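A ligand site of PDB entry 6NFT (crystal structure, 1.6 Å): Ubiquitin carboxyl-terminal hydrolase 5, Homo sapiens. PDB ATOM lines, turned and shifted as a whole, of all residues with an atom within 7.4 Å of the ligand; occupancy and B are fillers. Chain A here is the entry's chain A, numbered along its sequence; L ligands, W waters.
SD of Met 97 sits close to N1 of the ligand (3.6 Å).
Trp 40 touches the ligand.
CA of Gly 51 touches O3 of the ligand, 3.3 Å away.
Tyr 54 touches the ligand.
Ala 64 touches the ligand.
Val 65 touches the ligand.
CE1 of Tyr 90 touches C9 of the ligand, at 3.3 Å.
Hydrophobic or aromatic side chains within 4 Å of the ligand: Trp 40, Ala 64, Val 65, Tyr 90, Tyr 92 and Met 97.
Within 4 Å of the ligand: Trp 40, Gly 51, Arg 52, Tyr 54, Ala 64, Val 65, Tyr 90, Tyr 92 and Met 97.
The nearest printed residue that does not touch the ligand is Cys 50 (4.3 Å).
Water W1 bridges an oxygen (O3) of the ligand (2.7 Å) and the side-chain hydroxyl of Tyr 54 (2.8 Å).
The backbone carbonyl oxygen of Arg 52 lies within hydrogen-bond range of the backbone NH of Gly 60 (3.1 Å).
NH1 of Arg 52 sits at hydrogen-bond distance from OH of Tyr 90 (3.0 Å).
The indole nitrogen (NE1) of Trp 40 is in hydrogen-bond range of the side-chain amide oxygen (OD1) of Asn 38 (3.1 Å).
The backbone NH (N) of Tyr 90 sits at hydrogen-bond distance from the backbone carbonyl oxygen (O) of Ala 76 (2.8 Å).
The backbone carbonyl oxygen (O) of Gly 51 sits at hydrogen-bond distance from the backbone NH (N) of Asn 62 (3.1 Å).
The backbone carbonyl oxygen of Cys 50 lies within hydrogen-bond range of the backbone NH of Ala 64 (2.9 Å).
The backbone carbonyl oxygen (O) of Gly 51 sits close to the backbone NH (N) of Gly 60 (3.4 Å).
O of Leu 49 is in hydrogen-bond range of N of Trp 40 (2.8 Å).
OH of Tyr 92 is in hydrogen-bond range of O1 of the ligand, at 2.7 Å.
NE of Arg 52 sits at hydrogen-bond distance from O2 of the ligand (2.8 Å).
O3 of the ligand lies within hydrogen-bond range of N of Arg 52 (2.7 Å).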
ATOM      1  N   ASN A  38      12.210 -20.153   9.580  1.00  0.00           N
ATOM      2  CA  ASN A  38      11.532 -21.065   8.630  1.00  0.00           C
ATOM      3  C   ASN A  38      10.044 -21.173   8.986  1.00  0.00           C
ATOM      4  O   ASN A  38       9.514 -22.288   9.094  1.00  0.00           O
ATOM      5  CB  ASN A  38      12.206 -22.420   8.656  1.00  0.00           C
ATOM      6  CG  ASN A  38      11.821 -23.301   7.489  1.00  0.00           C
ATOM      7  OD1 ASN A  38      11.224 -22.801   6.511  1.00  0.00           O
ATOM      8  ND2 ASN A  38      12.158 -24.583   7.593  1.00  0.00           N
ATOM      9  N   TRP A  40       6.002 -20.148   8.112  1.00  0.00           N
ATOM     10  CA  TRP A  40       5.075 -19.989   6.984  1.00  0.00           C
ATOM     11  C   TRP A  40       3.707 -19.518   7.510  1.00  0.00           C
ATOM     12  O   TRP A  40       3.105 -20.199   8.338  1.00  0.00           O
ATOM     13  CB  TRP A  40       4.978 -21.298   6.160  1.00  0.00           C
ATOM     14  CG  TRP A  40       6.320 -21.595   5.559  1.00  0.00           C
ATOM     15  CD1 TRP A  40       7.399 -22.135   6.187  1.00  0.00           C
ATOM     16  CD2 TRP A  40       6.759 -21.238   4.237  1.00  0.00           C
ATOM     17  NE1 TRP A  40       8.475 -22.153   5.340  1.00  0.00           N
ATOM     18  CE2 TRP A  40       8.112 -21.606   4.140  1.00  0.00           C
ATOM     19  CE3 TRP A  40       6.144 -20.661   3.119  1.00  0.00           C
ATOM     20  CZ2 TRP A  40       8.852 -21.408   2.976  1.00  0.00           C
ATOM     21  CZ3 TRP A  40       6.872 -20.474   1.960  1.00  0.00           C
ATOM     22  CH2 TRP A  40       8.211 -20.875   1.893  1.00  0.00           C
ATOM     23  N   LEU A  49       3.340 -21.476  11.117  1.00  0.00           N
ATOM     24  CA  LEU A  49       3.820 -22.839  11.382  1.00  0.00           C
ATOM     25  C   LEU A  49       5.113 -23.099  10.622  1.00  0.00           C
ATOM     26  O   LEU A  49       5.339 -22.506   9.528  1.00  0.00           O
ATOM     27  CB  LEU A  49       2.727 -23.822  10.973  1.00  0.00           C
ATOM     28  CG  LEU A  49       1.406 -23.703  11.713  1.00  0.00           C
ATOM     29  CD1 LEU A  49       0.298 -24.450  10.982  1.00  0.00           C
ATOM     30  CD2 LEU A  49       1.560 -24.214  13.138  1.00  0.00           C
ATOM     31  N   CYS A  50       5.943 -23.967  11.183  1.00  0.00           N
ATOM     32  CA  CYS A  50       7.301 -24.205  10.641  1.00  0.00           C
ATOM     33  C   CYS A  50       7.281 -25.026   9.333  1.00  0.00           C
ATOM     34  O   CYS A  50       6.339 -25.744   9.030  1.00  0.00           O
ATOM     35  CB  CYS A  50       8.194 -24.798  11.706  1.00  0.00           C
ATOM     36  SG  CYS A  50       7.640 -26.426  12.254  1.00  0.00           S
ATOM     37  N   GLY A  51       8.379 -24.860   8.589  1.00  0.00           N
ATOM     38  CA  GLY A  51       8.612 -25.400   7.252  1.00  0.00           C
ATOM     39  C   GLY A  51       8.858 -26.904   7.248  1.00  0.00           C
ATOM     40  O   GLY A  51       9.018 -27.545   8.308  1.00  0.00           O
ATOM     41  N   ARG A  52       8.845 -27.462   6.046  1.00  0.00           N
ATOM     42  CA  ARG A  52       8.970 -28.918   5.845  1.00  0.00           C
ATOM     43  C   ARG A  52      10.296 -29.461   6.382  1.00  0.00           C
ATOM     44  O   ARG A  52      11.334 -28.793   6.247  1.00  0.00           O
ATOM     45  CB  ARG A  52       8.881 -29.191   4.344  1.00  0.00           C
ATOM     46  CG  ARG A  52       8.358 -30.590   4.085  1.00  0.00           C
ATOM     47  CD  ARG A  52       8.279 -30.823   2.613  1.00  0.00           C
ATOM     48  NE  ARG A  52       7.205 -30.122   1.947  1.00  0.00           N
ATOM     49  CZ  ARG A  52       6.112 -30.694   1.491  1.00  0.00           C
ATOM     50  NH1 ARG A  52       5.245 -29.941   0.858  1.00  0.00           N
ATOM     51  NH2 ARG A  52       5.867 -31.976   1.709  1.00  0.00           N
ATOM     52  N   ARG A  53      10.253 -30.681   6.912  1.00  0.00           N
ATOM     53  CA  ARG A  53      11.451 -31.525   7.086  1.00  0.00           C
ATOM     54  C   ARG A  53      11.747 -32.168   5.746  1.00  0.00           C
ATOM     55  O   ARG A  53      10.913 -32.983   5.257  1.00  0.00           O
ATOM     56  CB  ARG A  53      11.233 -32.575   8.174  1.00  0.00           C
ATOM     57  CG  ARG A  53      12.449 -33.430   8.463  1.00  0.00           C
ATOM     58  CD  ARG A  53      13.524 -32.641   9.192  1.00  0.00           C
ATOM     59  NE  ARG A  53      13.047 -32.183  10.483  1.00  0.00           N
ATOM     60  CZ  ARG A  53      12.835 -32.962  11.538  1.00  0.00           C
ATOM     61  NH1 ARG A  53      13.104 -34.259  11.484  1.00  0.00           N
ATOM     62  NH2 ARG A  53      12.374 -32.440  12.651  1.00  0.00           N
ATOM     63  N   TYR A  54      12.922 -31.887   5.185  1.00  0.00           N
ATOM     64  CA  TYR A  54      13.395 -32.489   3.917  1.00  0.00           C
ATOM     65  C   TYR A  54      13.982 -33.888   4.209  1.00  0.00           C
ATOM     66  O   TYR A  54      14.299 -34.215   5.364  1.00  0.00           O
ATOM     67  CB  TYR A  54      14.363 -31.547   3.225  1.00  0.00           C
ATOM     68  CG  TYR A  54      13.729 -30.293   2.704  1.00  0.00           C
ATOM     69  CD1 TYR A  54      12.793 -30.349   1.689  1.00  0.00           C
ATOM     70  CD2 TYR A  54      14.061 -29.048   3.203  1.00  0.00           C
ATOM     71  CE1 TYR A  54      12.172 -29.214   1.203  1.00  0.00           C
ATOM     72  CE2 TYR A  54      13.424 -27.899   2.745  1.00  0.00           C
ATOM     73  CZ  TYR A  54      12.465 -27.982   1.750  1.00  0.00           C
ATOM     74  OH  TYR A  54      11.849 -26.858   1.237  1.00  0.00           O
ATOM     75  N   GLY A  60      12.356 -27.651   8.896  1.00  0.00           N
ATOM     76  CA  GLY A  60      11.618 -27.544  10.152  1.00  0.00           C
ATOM     77  C   GLY A  60      10.973 -28.843  10.607  1.00  0.00           C
ATOM     78  O   GLY A  60      11.487 -29.952  10.284  1.00  0.00           O
ATOM     79  N   ASN A  62       7.693 -29.673  10.061  1.00  0.00           N
ATOM     80  CA  ASN A  62       6.585 -30.044   9.136  1.00  0.00           C
ATOM     81  C   ASN A  62       5.239 -29.555   9.637  1.00  0.00           C
ATOM     82  O   ASN A  62       4.224 -30.095   9.194  1.00  0.00           O
ATOM     83  CB  ASN A  62       6.423 -31.558   9.031  1.00  0.00           C
ATOM     84  CG  ASN A  62       7.417 -32.127   8.059  1.00  0.00           C
ATOM     85  OD1 ASN A  62       7.459 -31.728   6.890  1.00  0.00           O
ATOM     86  ND2 ASN A  62       8.141 -33.102   8.561  1.00  0.00           N
ATOM     87  N   HIS A  63       5.187 -28.597  10.546  1.00  0.00           N
ATOM     88  CA  HIS A  63       3.884 -28.189  11.131  1.00  0.00           C
ATOM     89  C   HIS A  63       3.022 -27.491  10.090  1.00  0.00           C
ATOM     90  O   HIS A  63       1.806 -27.722  10.082  1.00  0.00           O
ATOM     91  CB  HIS A  63       4.074 -27.360  12.386  1.00  0.00           C
ATOM     92  CG  HIS A  63       4.534 -28.220  13.489  1.00  0.00           C
ATOM     93  ND1 HIS A  63       5.589 -27.884  14.343  1.00  0.00           N
ATOM     94  CD2 HIS A  63       4.115 -29.456  13.838  1.00  0.00           C
ATOM     95  CE1 HIS A  63       5.759 -28.870  15.195  1.00  0.00           C
ATOM     96  NE2 HIS A  63       4.862 -29.850  14.906  1.00  0.00           N
ATOM     97  N   ALA A  64       3.587 -26.702   9.190  1.00  0.00           N
ATOM     98  CA  ALA A  64       2.797 -26.054   8.148  1.00  0.00           C
ATOM     99  C   ALA A  64       2.213 -27.116   7.186  1.00  0.00           C
ATOM    100  O   ALA A  64       1.042 -26.994   6.842  1.00  0.00           O
ATOM    101  CB  ALA A  64       3.616 -24.984   7.470  1.00  0.00           C
ATOM    102  N   VAL A  65       2.996 -28.109   6.770  1.00  0.00           N
ATOM    103  CA  VAL A  65       2.499 -29.166   5.853  1.00  0.00           C
ATOM    104  C   VAL A  65       1.395 -29.964   6.566  1.00  0.00           C
ATOM    105  O   VAL A  65       0.391 -30.239   5.925  1.00  0.00           O
ATOM    106  CB  VAL A  65       3.622 -30.088   5.336  1.00  0.00           C
ATOM    107  CG1 VAL A  65       4.507 -29.389   4.328  1.00  0.00           C
ATOM    108  CG2 VAL A  65       4.437 -30.687   6.454  1.00  0.00           C
ATOM    109  N   GLU A  66       1.557 -30.261   7.857  1.00  0.00           N
ATOM    110  CA  GLU A  66       0.530 -31.053   8.616  1.00  0.00           C
ATOM    111  C   GLU A  66      -0.766 -30.242   8.668  1.00  0.00           C
ATOM    112  O   GLU A  66      -1.881 -30.823   8.570  1.00  0.00           O
ATOM    113  CB  GLU A  66       1.102 -31.435   9.996  1.00  0.00           C
ATOM    114  CG  GLU A  66       2.180 -32.491   9.825  1.00  0.00           C
ATOM    115  CD  GLU A  66       2.959 -32.947  11.040  1.00  0.00           C
ATOM    116  OE1 GLU A  66       2.655 -32.444  12.121  1.00  0.00           O
ATOM    117  OE2 GLU A  66       3.864 -33.830  10.870  1.00  0.00           O
ATOM    118  N   ALA A  76       0.845 -20.400   1.375  1.00  0.00           N
ATOM    119  CA  ALA A  76       1.519 -19.843   2.550  1.00  0.00           C
ATOM    120  C   ALA A  76       2.686 -18.979   2.085  1.00  0.00           C
ATOM    121  O   ALA A  76       3.331 -19.320   1.074  1.00  0.00           O
ATOM    122  CB  ALA A  76       1.939 -20.909   3.506  1.00  0.00           C
ATOM    123  N   LYS A  78       6.447 -17.176   3.291  1.00  0.00           N
ATOM    124  CA  LYS A  78       7.535 -17.327   4.268  1.00  0.00           C
ATOM    125  C   LYS A  78       7.739 -15.988   4.973  1.00  0.00           C
ATOM    126  O   LYS A  78       8.154 -15.027   4.337  1.00  0.00           O
ATOM    127  CB  LYS A  78       8.848 -17.771   3.635  1.00  0.00           C
ATOM    128  CG  LYS A  78       9.858 -18.209   4.670  1.00  0.00           C
ATOM    129  CD  LYS A  78      11.148 -18.700   4.103  1.00  0.00           C
ATOM    130  CE  LYS A  78      11.976 -19.457   5.118  1.00  0.00           C
ATOM    131  NZ  LYS A  78      13.277 -19.869   4.520  1.00  0.00           N
ATOM    132  N   ASP A  88       8.279 -15.046  -0.829  1.00  0.00           N
ATOM    133  CA  ASP A  88       8.305 -16.491  -1.134  1.00  0.00           C
ATOM    134  C   ASP A  88       6.917 -17.045  -0.803  1.00  0.00           C
ATOM    135  O   ASP A  88       6.550 -17.113   0.384  1.00  0.00           O
ATOM    136  CB  ASP A  88       9.432 -17.211  -0.401  1.00  0.00           C
ATOM    137  CG  ASP A  88      10.815 -16.921  -0.937  1.00  0.00           C
ATOM    138  OD1 ASP A  88      10.919 -16.359  -2.078  1.00  0.00           O
ATOM    139  OD2 ASP A  88      11.777 -17.296  -0.246  1.00  0.00           O
ATOM    140  N   VAL A  89       6.177 -17.419  -1.830  1.00  0.00           N
ATOM    141  CA  VAL A  89       4.822 -17.997  -1.663  1.00  0.00           C
ATOM    142  C   VAL A  89       4.863 -19.441  -2.154  1.00  0.00           C
ATOM    143  O   VAL A  89       5.334 -19.662  -3.296  1.00  0.00           O
ATOM    144  CB  VAL A  89       3.744 -17.180  -2.387  1.00  0.00           C
ATOM    145  CG1 VAL A  89       2.367 -17.758  -2.110  1.00  0.00           C
ATOM    146  CG2 VAL A  89       3.763 -15.719  -1.943  1.00  0.00           C
ATOM    147  N   TYR A  90       4.429 -20.383  -1.301  1.00  0.00           N
ATOM    148  CA  TYR A  90       4.400 -21.817  -1.678  1.00  0.00           C
ATOM    149  C   TYR A  90       2.945 -22.259  -1.767  1.00  0.00           C
ATOM    150  O   TYR A  90       2.138 -21.814  -0.961  1.00  0.00           O
ATOM    151  CB  TYR A  90       5.221 -22.656  -0.700  1.00  0.00           C
ATOM    152  CG  TYR A  90       5.310 -24.120  -1.068  1.00  0.00           C
ATOM    153  CD1 TYR A  90       6.177 -24.670  -2.020  1.00  0.00           C
ATOM    154  CD2 TYR A  90       4.471 -24.971  -0.369  1.00  0.00           C
ATOM    155  CE1 TYR A  90       6.158 -26.049  -2.274  1.00  0.00           C
ATOM    156  CE2 TYR A  90       4.441 -26.306  -0.615  1.00  0.00           C
ATOM    157  CZ  TYR A  90       5.291 -26.852  -1.542  1.00  0.00           C
ATOM    158  OH  TYR A  90       5.119 -28.208  -1.621  1.00  0.00           O
ATOM    159  N   SER A  91       2.622 -23.121  -2.730  1.00  0.00           N
ATOM    160  CA  SER A  91       1.303 -23.800  -2.860  1.00  0.00           C
ATOM    161  C   SER A  91       1.477 -25.266  -2.485  1.00  0.00           C
ATOM    162  O   SER A  91       2.207 -26.011  -3.206  1.00  0.00           O
ATOM    163  CB  SER A  91       0.777 -23.658  -4.271  1.00  0.00           C
ATOM    164  OG  SER A  91      -0.381 -24.452  -4.421  1.00  0.00           O
ATOM    165  N   TYR A  92       0.833 -25.728  -1.428  1.00  0.00           N
ATOM    166  CA  TYR A  92       0.891 -27.164  -1.039  1.00  0.00           C
ATOM    167  C   TYR A  92       0.146 -28.014  -2.071  1.00  0.00           C
ATOM    168  O   TYR A  92       0.541 -29.143  -2.314  1.00  0.00           O
ATOM    169  CB  TYR A  92       0.300 -27.330   0.357  1.00  0.00           C
ATOM    170  CG  TYR A  92       1.136 -26.667   1.414  1.00  0.00           C
ATOM    171  CD1 TYR A  92       2.339 -27.209   1.833  1.00  0.00           C
ATOM    172  CD2 TYR A  92       0.752 -25.459   1.977  1.00  0.00           C
ATOM    173  CE1 TYR A  92       3.129 -26.588   2.805  1.00  0.00           C
ATOM    174  CE2 TYR A  92       1.534 -24.820   2.936  1.00  0.00           C
ATOM    175  CZ  TYR A  92       2.700 -25.408   3.378  1.00  0.00           C
ATOM    176  OH  TYR A  92       3.514 -24.732   4.266  1.00  0.00           O
ATOM    177  N   ASP A  95       2.261 -27.987  -5.117  1.00  0.00           N
ATOM    178  CA  ASP A  95       3.601 -28.444  -4.705  1.00  0.00           C
ATOM    179  C   ASP A  95       4.666 -27.698  -5.507  1.00  0.00           C
ATOM    180  O   ASP A  95       5.577 -28.338  -6.127  1.00  0.00           O
ATOM    181  CB  ASP A  95       3.721 -29.964  -4.836  1.00  0.00           C
ATOM    182  CG  ASP A  95       4.940 -30.553  -4.143  1.00  0.00           C
ATOM    183  OD1 ASP A  95       5.537 -29.872  -3.285  1.00  0.00           O
ATOM    184  OD2 ASP A  95       5.293 -31.698  -4.481  1.00  0.00           O
ATOM    185  N   ASP A  96       4.655 -26.366  -5.384  1.00  0.00           N
ATOM    186  CA  ASP A  96       5.630 -25.497  -6.065  1.00  0.00           C
ATOM    187  C   ASP A  96       5.630 -24.134  -5.413  1.00  0.00           C
ATOM    188  O   ASP A  96       4.590 -23.733  -4.844  1.00  0.00           O
ATOM    189  CB  ASP A  96       5.309 -25.365  -7.559  1.00  0.00           C
ATOM    190  CG  ASP A  96       6.042 -26.339  -8.469  1.00  0.00           C
ATOM    191  OD1 ASP A  96       7.286 -26.537  -8.291  1.00  0.00           O
ATOM    192  OD2 ASP A  96       5.366 -26.888  -9.333  1.00  0.00           O
ATOM    193  N   MET A  97       6.737 -23.428  -5.543  1.00  0.00           N
ATOM    194  CA  MET A  97       6.777 -21.993  -5.276  1.00  0.00           C
ATOM    195  C   MET A  97       5.951 -21.341  -6.381  1.00  0.00           C
ATOM    196  O   MET A  97       6.062 -21.788  -7.567  1.00  0.00           O
ATOM    197  CB  MET A  97       8.186 -21.412  -5.300  1.00  0.00           C
ATOM    198  CG  MET A  97       9.173 -22.093  -4.383  1.00  0.00           C
ATOM    199  SD  MET A  97       8.648 -22.003  -2.643  1.00  0.00           S
ATOM    200  CE  MET A  97       8.288 -20.281  -2.420  1.00  0.00           C
HETATM  201  C1  LIG L   1       6.771 -25.602   3.900  1.00  0.00           C
HETATM  202  C2  LIG L   1       8.141 -24.125   1.101  1.00  0.00           C
HETATM  203  C3  LIG L   1       9.211 -25.406  -0.441  1.00  0.00           C
HETATM  204  C4  LIG L   1      10.123 -25.501  -1.486  1.00  0.00           C
HETATM  205  C5  LIG L   1      10.345 -26.724  -2.109  1.00  0.00           C
HETATM  206  C6  LIG L   1       9.688 -27.849  -1.687  1.00  0.00           C
HETATM  207  O1  LIG L   1       5.900 -25.963   4.719  1.00  0.00           O
HETATM  208  O2  LIG L   1       6.820 -27.347   1.446  1.00  0.00           O
HETATM  209  N1  LIG L   1       9.030 -24.177   0.174  1.00  0.00           N
HETATM  210  C7  LIG L   1       7.499 -26.435   1.016  1.00  0.00           C
HETATM  211  N2  LIG L   1       7.360 -25.150   1.536  1.00  0.00           N
HETATM  212  C8  LIG L   1       6.369 -24.941   2.588  1.00  0.00           C
HETATM  213  O3  LIG L   1       8.000 -25.855   4.009  1.00  0.00           O
HETATM  214  C9  LIG L   1       8.518 -26.549  -0.038  1.00  0.00           C
HETATM  215  C10 LIG L   1       8.780 -27.783  -0.656  1.00  0.00           C
HETATM  216  O   HOH W   1      10.534 -25.337   3.216  1.00  0.00           O
HETATM  217  O   HOH W   2      11.369 -22.528   0.149  1.00  0.00           O
HETATM  218  O   HOH W   3       5.853 -27.656   7.118  1.00  0.00           O
